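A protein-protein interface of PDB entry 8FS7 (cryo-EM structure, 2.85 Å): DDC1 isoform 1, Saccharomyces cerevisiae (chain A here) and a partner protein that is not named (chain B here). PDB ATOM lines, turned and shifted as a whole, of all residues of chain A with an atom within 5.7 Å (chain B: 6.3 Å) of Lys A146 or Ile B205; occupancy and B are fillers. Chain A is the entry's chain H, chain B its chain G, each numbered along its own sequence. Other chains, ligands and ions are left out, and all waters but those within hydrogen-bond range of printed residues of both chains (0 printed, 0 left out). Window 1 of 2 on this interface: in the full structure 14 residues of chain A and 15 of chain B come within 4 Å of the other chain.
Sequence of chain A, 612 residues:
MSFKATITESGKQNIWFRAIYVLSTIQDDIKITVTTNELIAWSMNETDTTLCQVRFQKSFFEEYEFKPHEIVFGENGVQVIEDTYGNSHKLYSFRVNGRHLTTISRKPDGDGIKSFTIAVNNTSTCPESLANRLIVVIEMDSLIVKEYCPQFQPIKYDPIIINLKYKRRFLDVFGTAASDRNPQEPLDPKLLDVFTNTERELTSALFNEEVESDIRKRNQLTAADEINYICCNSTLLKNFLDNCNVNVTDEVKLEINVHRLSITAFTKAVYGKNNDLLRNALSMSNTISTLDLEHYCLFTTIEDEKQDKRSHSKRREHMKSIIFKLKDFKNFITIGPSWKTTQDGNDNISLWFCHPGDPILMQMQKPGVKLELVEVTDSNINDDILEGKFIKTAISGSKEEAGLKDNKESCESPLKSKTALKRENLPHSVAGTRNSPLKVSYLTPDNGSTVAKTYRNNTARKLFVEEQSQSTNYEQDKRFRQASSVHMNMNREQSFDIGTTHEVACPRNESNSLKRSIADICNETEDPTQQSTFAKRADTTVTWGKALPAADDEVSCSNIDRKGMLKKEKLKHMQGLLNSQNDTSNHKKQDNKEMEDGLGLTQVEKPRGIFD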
ATOM      1  N   ARG A 106     -16.444  -9.565  23.967  1.00  0.00           N
ATOM      2  CA  ARG A 106     -16.667 -10.791  23.219  1.00  0.00           C
ATOM      3  C   ARG A 106     -16.872 -10.489  21.737  1.00  0.00           C
ATOM      4  O   ARG A 106     -17.372  -9.428  21.350  1.00  0.00           O
ATOM      5  CB  ARG A 106     -17.880 -11.541  23.766  1.00  0.00           C
ATOM      6  CG  ARG A 106     -19.014 -10.631  24.201  1.00  0.00           C
ATOM      7  CD  ARG A 106     -20.362 -11.310  24.051  1.00  0.00           C
ATOM      8  NE  ARG A 106     -20.841 -11.255  22.674  1.00  0.00           N
ATOM      9  CZ  ARG A 106     -21.528 -10.245  22.161  1.00  0.00           C
ATOM     10  NH1 ARG A 106     -21.839  -9.181  22.885  1.00  0.00           N
ATOM     11  NH2 ARG A 106     -21.912 -10.301  20.889  1.00  0.00           N
ATOM     12  N   PRO A 108     -18.843 -10.928  18.470  1.00  0.00           N
ATOM     13  CA  PRO A 108     -20.161 -11.384  18.014  1.00  0.00           C
ATOM     14  C   PRO A 108     -20.040 -12.357  16.851  1.00  0.00           C
ATOM     15  O   PRO A 108     -19.107 -12.291  16.048  1.00  0.00           O
ATOM     16  CB  PRO A 108     -20.861 -10.087  17.587  1.00  0.00           C
ATOM     17  CG  PRO A 108     -20.092  -8.989  18.262  1.00  0.00           C
ATOM     18  CD  PRO A 108     -18.679  -9.474  18.312  1.00  0.00           C
ATOM     19  N   VAL A 136     -16.349   2.399  26.740  1.00  0.00           N
ATOM     20  CA  VAL A 136     -15.861   1.444  25.754  1.00  0.00           C
ATOM     21  C   VAL A 136     -16.735   1.562  24.513  1.00  0.00           C
ATOM     22  O   VAL A 136     -17.962   1.467  24.604  1.00  0.00           O
ATOM     23  CB  VAL A 136     -15.865   0.002  26.296  1.00  0.00           C
ATOM     24  CG1 VAL A 136     -17.088  -0.244  27.173  1.00  0.00           C
ATOM     25  CG2 VAL A 136     -15.800  -1.001  25.154  1.00  0.00           C
ATOM     26  N   VAL A 137     -16.104   1.775  23.360  1.00  0.00           N
ATOM     27  CA  VAL A 137     -16.802   1.961  22.092  1.00  0.00           C
ATOM     28  C   VAL A 137     -16.367   0.857  21.140  1.00  0.00           C
ATOM     29  O   VAL A 137     -15.167   0.630  20.950  1.00  0.00           O
ATOM     30  CB  VAL A 137     -16.521   3.347  21.486  1.00  0.00           C
ATOM     31  CG1 VAL A 137     -17.245   3.507  20.157  1.00  0.00           C
ATOM     32  CG2 VAL A 137     -16.925   4.447  22.456  1.00  0.00           C
ATOM     33  N   ILE A 138     -17.341   0.173  20.542  1.00  0.00           N
ATOM     34  CA  ILE A 138     -17.090  -0.899  19.586  1.00  0.00           C
ATOM     35  C   ILE A 138     -17.734  -0.532  18.258  1.00  0.00           C
ATOM     36  O   ILE A 138     -18.928  -0.219  18.205  1.00  0.00           O
ATOM     37  CB  ILE A 138     -17.617  -2.253  20.093  1.00  0.00           C
ATOM     38  CG1 ILE A 138     -16.879  -2.660  21.364  1.00  0.00           C
ATOM     39  CG2 ILE A 138     -17.477  -3.321  19.019  1.00  0.00           C
ATOM     40  CD1 ILE A 138     -17.774  -2.958  22.525  1.00  0.00           C
ATOM     41  N   GLU A 139     -16.941  -0.576  17.192  1.00  0.00           N
ATOM     42  CA  GLU A 139     -17.414  -0.355  15.832  1.00  0.00           C
ATOM     43  C   GLU A 139     -17.273  -1.658  15.058  1.00  0.00           C
ATOM     44  O   GLU A 139     -16.163  -2.179  14.912  1.00  0.00           O
ATOM     45  CB  GLU A 139     -16.626   0.766  15.155  1.00  0.00           C
ATOM     46  CG  GLU A 139     -17.330   1.397  13.968  1.00  0.00           C
ATOM     47  CD  GLU A 139     -16.908   2.835  13.743  1.00  0.00           C
ATOM     48  OE1 GLU A 139     -16.268   3.416  14.646  1.00  0.00           O
ATOM     49  OE2 GLU A 139     -17.213   3.386  12.665  1.00  0.00           O
ATOM     50  N   MET A 140     -18.394  -2.185  14.574  1.00  0.00           N
ATOM     51  CA  MET A 140     -18.371  -3.426  13.818  1.00  0.00           C
ATOM     52  C   MET A 140     -18.001  -3.164  12.362  1.00  0.00           C
ATOM     53  O   MET A 140     -17.937  -2.021  11.903  1.00  0.00           O
ATOM     54  CB  MET A 140     -19.725  -4.133  13.901  1.00  0.00           C
ATOM     55  CG  MET A 140     -20.399  -4.028  15.260  1.00  0.00           C
ATOM     56  SD  MET A 140     -19.643  -5.041  16.551  1.00  0.00           S
ATOM     57  CE  MET A 140     -19.034  -6.443  15.617  1.00  0.00           C
ATOM     58  N   ILE A 144     -22.099  -0.658  12.447  1.00  0.00           N
ATOM     59  CA  ILE A 144     -22.942  -0.511  13.627  1.00  0.00           C
ATOM     60  C   ILE A 144     -22.063  -0.156  14.818  1.00  0.00           C
ATOM     61  O   ILE A 144     -21.080  -0.847  15.111  1.00  0.00           O
ATOM     62  CB  ILE A 144     -23.747  -1.795  13.889  1.00  0.00           C
ATOM     63  CG1 ILE A 144     -24.460  -2.239  12.609  1.00  0.00           C
ATOM     64  CG2 ILE A 144     -24.717  -1.597  15.045  1.00  0.00           C
ATOM     65  CD1 ILE A 144     -24.903  -3.682  12.617  1.00  0.00           C
ATOM     66  N   VAL A 145     -22.410   0.928  15.506  1.00  0.00           N
ATOM     67  CA  VAL A 145     -21.651   1.412  16.652  1.00  0.00           C
ATOM     68  C   VAL A 145     -22.383   1.006  17.921  1.00  0.00           C
ATOM     69  O   VAL A 145     -23.555   1.353  18.110  1.00  0.00           O
ATOM     70  CB  VAL A 145     -21.446   2.936  16.595  1.00  0.00           C
ATOM     71  CG1 VAL A 145     -20.485   3.380  17.685  1.00  0.00           C
ATOM     72  CG2 VAL A 145     -20.928   3.351  15.225  1.00  0.00           C
ATOM     73  N   LYS A 146     -21.693   0.262  18.781  1.00  0.00           N
ATOM     74  CA  LYS A 146     -22.208  -0.140  20.084  1.00  0.00           C
ATOM     75  C   LYS A 146     -21.198   0.298  21.133  1.00  0.00           C
ATOM     76  O   LYS A 146     -20.029  -0.093  21.066  1.00  0.00           O
ATOM     77  CB  LYS A 146     -22.417  -1.654  20.156  1.00  0.00           C
ATOM     78  CG  LYS A 146     -22.979  -2.281  18.895  1.00  0.00           C
ATOM     79  CD  LYS A 146     -22.945  -3.795  18.994  1.00  0.00           C
ATOM     80  CE  LYS A 146     -21.565  -4.277  19.422  1.00  0.00           C
ATOM     81  NZ  LYS A 146     -21.499  -5.755  19.595  1.00  0.00           N
ATOM     82  N   GLU A 147     -21.638   1.107  22.093  1.00  0.00           N
ATOM     83  CA  GLU A 147     -20.773   1.552  23.176  1.00  0.00           C
ATOM     84  C   GLU A 147     -21.492   1.405  24.511  1.00  0.00           C
ATOM     85  O   GLU A 147     -22.718   1.552  24.582  1.00  0.00           O
ATOM     86  CB  GLU A 147     -20.294   2.994  22.948  1.00  0.00           C
ATOM     87  CG  GLU A 147     -21.236   4.099  23.385  1.00  0.00           C
ATOM     88  CD  GLU A 147     -21.780   4.888  22.210  1.00  0.00           C
ATOM     89  OE1 GLU A 147     -21.935   6.120  22.341  1.00  0.00           O
ATOM     90  OE2 GLU A 147     -22.062   4.279  21.157  1.00  0.00           O
ATOM     91  N   TYR A 148     -20.727   1.096  25.558  1.00  0.00           N
ATOM     92  CA  TYR A 148     -21.249   0.819  26.887  1.00  0.00           C
ATOM     93  C   TYR A 148     -20.631   1.777  27.898  1.00  0.00           C
ATOM     94  O   TYR A 148     -19.608   2.414  27.635  1.00  0.00           O
ATOM     95  CB  TYR A 148     -20.948  -0.622  27.325  1.00  0.00           C
ATOM     96  CG  TYR A 148     -21.290  -1.678  26.299  1.00  0.00           C
ATOM     97  CD1 TYR A 148     -20.381  -2.039  25.320  1.00  0.00           C
ATOM     98  CD2 TYR A 148     -22.509  -2.329  26.326  1.00  0.00           C
ATOM     99  CE1 TYR A 148     -20.688  -3.005  24.381  1.00  0.00           C
ATOM    100  CE2 TYR A 148     -22.830  -3.293  25.390  1.00  0.00           C
ATOM    101  CZ  TYR A 148     -21.913  -3.628  24.422  1.00  0.00           C
ATOM    102  OH  TYR A 148     -22.228  -4.595  23.494  1.00  0.00           O
ATOM    103  N   ALA B 162     -28.714  -6.727  10.712  1.00  0.00           N
ATOM    104  CA  ALA B 162     -28.263  -5.738  11.688  1.00  0.00           C
ATOM    105  C   ALA B 162     -29.175  -5.704  12.909  1.00  0.00           C
ATOM    106  O   ALA B 162     -28.697  -5.637  14.049  1.00  0.00           O
ATOM    107  CB  ALA B 162     -28.185  -4.358  11.036  1.00  0.00           C
ATOM    108  N   SER B 165     -28.518  -8.792  14.990  1.00  0.00           N
ATOM    109  CA  SER B 165     -27.276  -8.655  15.745  1.00  0.00           C
ATOM    110  C   SER B 165     -27.459  -7.734  16.946  1.00  0.00           C
ATOM    111  O   SER B 165     -26.967  -8.026  18.045  1.00  0.00           O
ATOM    112  CB  SER B 165     -26.162  -8.138  14.835  1.00  0.00           C
ATOM    113  OG  SER B 165     -26.505  -6.885  14.271  1.00  0.00           O
ATOM    114  N   ALA B 166     -28.169  -6.618  16.756  1.00  0.00           N
ATOM    115  CA  ALA B 166     -28.432  -5.707  17.866  1.00  0.00           C
ATOM    116  C   ALA B 166     -29.268  -6.380  18.949  1.00  0.00           C
ATOM    117  O   ALA B 166     -28.990  -6.226  20.145  1.00  0.00           O
ATOM    118  CB  ALA B 166     -29.127  -4.445  17.357  1.00  0.00           C
ATOM    119  N   LEU B 167     -30.294  -7.135  18.548  1.00  0.00           N
ATOM    120  CA  LEU B 167     -31.133  -7.833  19.516  1.00  0.00           C
ATOM    121  C   LEU B 167     -30.340  -8.890  20.275  1.00  0.00           C
ATOM    122  O   LEU B 167     -30.513  -9.056  21.488  1.00  0.00           O
ATOM    123  CB  LEU B 167     -32.333  -8.465  18.811  1.00  0.00           C
ATOM    124  CG  LEU B 167     -33.674  -7.733  18.916  1.00  0.00           C
ATOM    125  CD1 LEU B 167     -34.171  -7.722  20.353  1.00  0.00           C
ATOM    126  CD2 LEU B 167     -33.568  -6.317  18.369  1.00  0.00           C
ATOM    127  N   ASP B 169     -27.068  -8.855  20.853  1.00  0.00           N
ATOM    128  CA  ASP B 169     -26.176  -8.164  21.780  1.00  0.00           C
ATOM    129  C   ASP B 169     -26.935  -7.642  22.993  1.00  0.00           C
ATOM    130  O   ASP B 169     -26.418  -7.674  24.117  1.00  0.00           O
ATOM    131  CB  ASP B 169     -25.451  -7.019  21.075  1.00  0.00           C
ATOM    132  CG  ASP B 169     -24.253  -6.525  21.863  1.00  0.00           C
ATOM    133  OD1 ASP B 169     -23.806  -7.244  22.781  1.00  0.00           O
ATOM    134  OD2 ASP B 169     -23.767  -5.412  21.578  1.00  0.00           O
ATOM    135  N   LEU B 170     -28.157  -7.142  22.788  1.00  0.00           N
ATOM    136  CA  LEU B 170     -28.979  -6.720  23.918  1.00  0.00           C
ATOM    137  C   LEU B 170     -29.305  -7.897  24.829  1.00  0.00           C
ATOM    138  O   LEU B 170     -29.268  -7.772  26.057  1.00  0.00           O
ATOM    139  CB  LEU B 170     -30.262  -6.056  23.419  1.00  0.00           C
ATOM    140  CG  LEU B 170     -30.146  -4.629  22.878  1.00  0.00           C
ATOM    141  CD1 LEU B 170     -31.520  -3.987  22.763  1.00  0.00           C
ATOM    142  CD2 LEU B 170     -29.230  -3.785  23.751  1.00  0.00           C
ATOM    143  N   PHE B 192     -30.934   6.003  14.519  1.00  0.00           N
ATOM    144  CA  PHE B 192     -31.776   4.997  15.158  1.00  0.00           C
ATOM    145  C   PHE B 192     -30.912   4.210  16.128  1.00  0.00           C
ATOM    146  O   PHE B 192     -29.935   3.577  15.715  1.00  0.00           O
ATOM    147  CB  PHE B 192     -32.416   4.070  14.119  1.00  0.00           C
ATOM    148  CG  PHE B 192     -33.538   3.233  14.663  1.00  0.00           C
ATOM    149  CD1 PHE B 192     -34.839   3.706  14.649  1.00  0.00           C
ATOM    150  CD2 PHE B 192     -33.296   1.973  15.182  1.00  0.00           C
ATOM    151  CE1 PHE B 192     -35.874   2.940  15.144  1.00  0.00           C
ATOM    152  CE2 PHE B 192     -34.327   1.201  15.678  1.00  0.00           C
ATOM    153  CZ  PHE B 192     -35.619   1.686  15.659  1.00  0.00           C
ATOM    154  N   ALA B 193     -31.266   4.249  17.410  1.00  0.00           N
ATOM    155  CA  ALA B 193     -30.474   3.601  18.444  1.00  0.00           C
ATOM    156  C   ALA B 193     -31.390   2.830  19.381  1.00  0.00           C
ATOM    157  O   ALA B 193     -32.579   3.129  19.508  1.00  0.00           O
ATOM    158  CB  ALA B 193     -29.639   4.616  19.234  1.00  0.00           C
ATOM    159  N   LEU B 194     -30.814   1.829  20.041  1.00  0.00           N
ATOM    160  CA  LEU B 194     -31.523   0.997  21.010  1.00  0.00           C
ATOM    161  C   LEU B 194     -30.850   1.176  22.367  1.00  0.00           C
ATOM    162  O   LEU B 194     -29.846   0.520  22.662  1.00  0.00           O
ATOM    163  CB  LEU B 194     -31.527  -0.467  20.577  1.00  0.00           C
ATOM    164  CG  LEU B 194     -32.381  -0.817  19.358  1.00  0.00           C
ATOM    165  CD1 LEU B 194     -32.123  -2.250  18.918  1.00  0.00           C
ATOM    166  CD2 LEU B 194     -33.857  -0.606  19.660  1.00  0.00           C
ATOM    167  N   ILE B 195     -31.401   2.064  23.189  1.00  0.00           N
ATOM    168  CA  ILE B 195     -30.896   2.300  24.536  1.00  0.00           C
ATOM    169  C   ILE B 195     -31.489   1.249  25.463  1.00  0.00           C
ATOM    170  O   ILE B 195     -32.683   0.942  25.391  1.00  0.00           O
ATOM    171  CB  ILE B 195     -31.231   3.725  25.014  1.00  0.00           C
ATOM    172  CG1 ILE B 195     -30.715   4.763  24.016  1.00  0.00           C
ATOM    173  CG2 ILE B 195     -30.625   3.981  26.383  1.00  0.00           C
ATOM    174  CD1 ILE B 195     -31.787   5.329  23.109  1.00  0.00           C
ATOM    175  N   SER B 203     -26.746   1.354  28.011  1.00  0.00           N
ATOM    176  CA  SER B 203     -26.211   0.679  26.841  1.00  0.00           C
ATOM    177  C   SER B 203     -26.967   1.138  25.609  1.00  0.00           C
ATOM    178  O   SER B 203     -28.198   1.121  25.598  1.00  0.00           O
ATOM    179  CB  SER B 203     -26.344  -0.833  26.970  1.00  0.00           C
ATOM    180  OG  SER B 203     -25.302  -1.486  26.289  1.00  0.00           O
ATOM    181  N   LYS B 204     -26.235   1.535  24.570  1.00  0.00           N
ATOM    182  CA  LYS B 204     -26.836   1.978  23.319  1.00  0.00           C
ATOM    183  C   LYS B 204     -26.244   1.211  22.144  1.00  0.00           C
ATOM    184  O   LYS B 204     -25.075   0.813  22.173  1.00  0.00           O
ATOM    185  CB  LYS B 204     -26.645   3.488  23.120  1.00  0.00           C
ATOM    186  CG  LYS B 204     -25.295   3.884  22.537  1.00  0.00           C
ATOM    187  CD  LYS B 204     -25.053   5.386  22.573  1.00  0.00           C
ATOM    188  CE  LYS B 204     -26.273   6.210  22.206  1.00  0.00           C
ATOM    189  NZ  LYS B 204     -26.913   5.796  20.924  1.00  0.00           N
ATOM    190  N   ILE B 205     -27.068   0.979  21.124  1.00  0.00           N
ATOM    191  CA  ILE B 205     -26.655   0.333  19.879  1.00  0.00           C
ATOM    192  C   ILE B 205     -27.271   1.154  18.755  1.00  0.00           C
ATOM    193  O   ILE B 205     -28.453   0.987  18.429  1.00  0.00           O
ATOM    194  CB  ILE B 205     -27.092  -1.136  19.803  1.00  0.00           C
ATOM    195  CG1 ILE B 205     -26.536  -1.935  20.990  1.00  0.00           C
ATOM    196  CG2 ILE B 205     -26.665  -1.758  18.466  1.00  0.00           C
ATOM    197  CD1 ILE B 205     -26.358  -3.419  20.727  1.00  0.00           C
ATOM    198  N   LYS B 206     -26.484   2.049  18.163  1.00  0.00           N
ATOM    199  CA  LYS B 206     -26.966   2.944  17.121  1.00  0.00           C
ATOM    200  C   LYS B 206     -26.683   2.343  15.749  1.00  0.00           C
ATOM    201  O   LYS B 206     -25.547   1.957  15.454  1.00  0.00           O
ATOM    202  CB  LYS B 206     -26.323   4.328  17.246  1.00  0.00           C
ATOM    203  CG  LYS B 206     -24.813   4.315  17.449  1.00  0.00           C
ATOM    204  CD  LYS B 206     -24.279   5.694  17.814  1.00  0.00           C
ATOM    205  CE  LYS B 206     -24.880   6.780  16.932  1.00  0.00           C
ATOM    206  NZ  LYS B 206     -24.616   6.554  15.481  1.00  0.00           N
ATOM    207  N   LEU B 207     -27.722   2.251  14.926  1.00  0.00           N
ATOM    208  CA  LEU B 207     -27.604   1.707  13.586  1.00  0.00           C
ATOM    209  C   LEU B 207     -26.986   2.735  12.639  1.00  0.00           C
ATOM    210  O   LEU B 207     -27.140   3.942  12.838  1.00  0.00           O
ATOM    211  CB  LEU B 207     -28.974   1.284  13.069  1.00  0.00           C
ATOM    212  CG  LEU B 207     -29.745   0.348  14.001  1.00  0.00           C
ATOM    213  CD1 LEU B 207     -31.057  -0.071  13.369  1.00  0.00           C
ATOM    214  CD2 LEU B 207     -28.901  -0.868  14.347  1.00  0.00           C
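Ala B162 touches Ile A144 (CB to CD1, 3.7 Å).
Ser B165 touches Ile A144 (OG to CD1, 3.9 Å).
Ile A144 touches Ile B205.
Ile A144 touches Lys B206 (CG2 to O, 3.7 Å).
Val A145 touches Ile B205.
O of Lys B204 touches CA of Lys A146 (3.7 Å).
Lys A146 touches Ile B205 (CG to CG2, 3.7 Å).
CD2 of Tyr A148 touches OG of Ser B203, at 2.9 Å.
O of Val A145 is in hydrogen-bond range of N of Lys B206.
OD1 of Asp B169 lies within salt-bridge range of NH1 of Arg A106, at 2.8 Å.
NZ of Lys A146 is in salt-bridge range of OD2 of Asp B169.
The backbone carbonyl oxygen of Lys B204 sits at hydrogen-bond distance from the backbone NH of Glu A147 (3.5 Å).
The side-chain carboxylate (OD2) of Asp B169 sits at hydrogen-bond distance from the side-chain hydroxyl (OH) of Tyr A148, 2.6 Å away.
Of the 15 printed residues of chain B, 7 touch a printed residue of chain A.
Of the 12 printed residues of chain A, 6 touch a printed residue of chain B.
Hydrophobic or aromatic side chains of chain A within 4 Å of the printed part of chain B: Ile A144, Val A145 and Tyr A148.
Among the printed residues, Asp or Glu carboxylates within 4 Å of a Lys or Arg side-chain nitrogen of the other chain: Arg A106 with Asp B169 (2.8 Å) and Lys A146 with Asp B169 (3.0 Å).
Glu A139 touches none of the printed residues of chain B.
Of chain B, only Asp B169 (3.0 Å), Lys B204 (3.7 Å) and Ile B205 (3.7 Å) come within 4 Å of Lys A146.
Of the printed residues of chain B, Glu A147 touches Lys B204 (3.2 Å).
Printed residues of chain A within 4 Å of Lys B204: Lys A146 and Glu A147.
Of chain A, only Ile A144 (3.9 Å), Val A145 (3.7 Å) and Lys A146 (3.7 Å) come within 4 Å of Ile B205.
The nearest residue of chain B that does not touch Lys A146 is Lys B206 (5.2 Å).
The backbone carbonyl oxygen of Lys A146 lies within hydrogen-bond range of the backbone NH of Ile A138 (2.8 Å).
The backbone NH (N) of Leu B194 sits at hydrogen-bond distance from the backbone carbonyl oxygen (O) of Ile B205.
O of Ala B162 sits at hydrogen-bond distance from OG of Ser B165, at 2.5 Å.
The backbone carbonyl oxygen (O) of Val A136 sits at hydrogen-bond distance from the backbone NH (N) of Tyr A148, 2.9 Å away.
The side-chain amino group (NZ) of Lys A146 sits close to the side-chain sulfur (SD) of Met A140 (3.6 Å).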
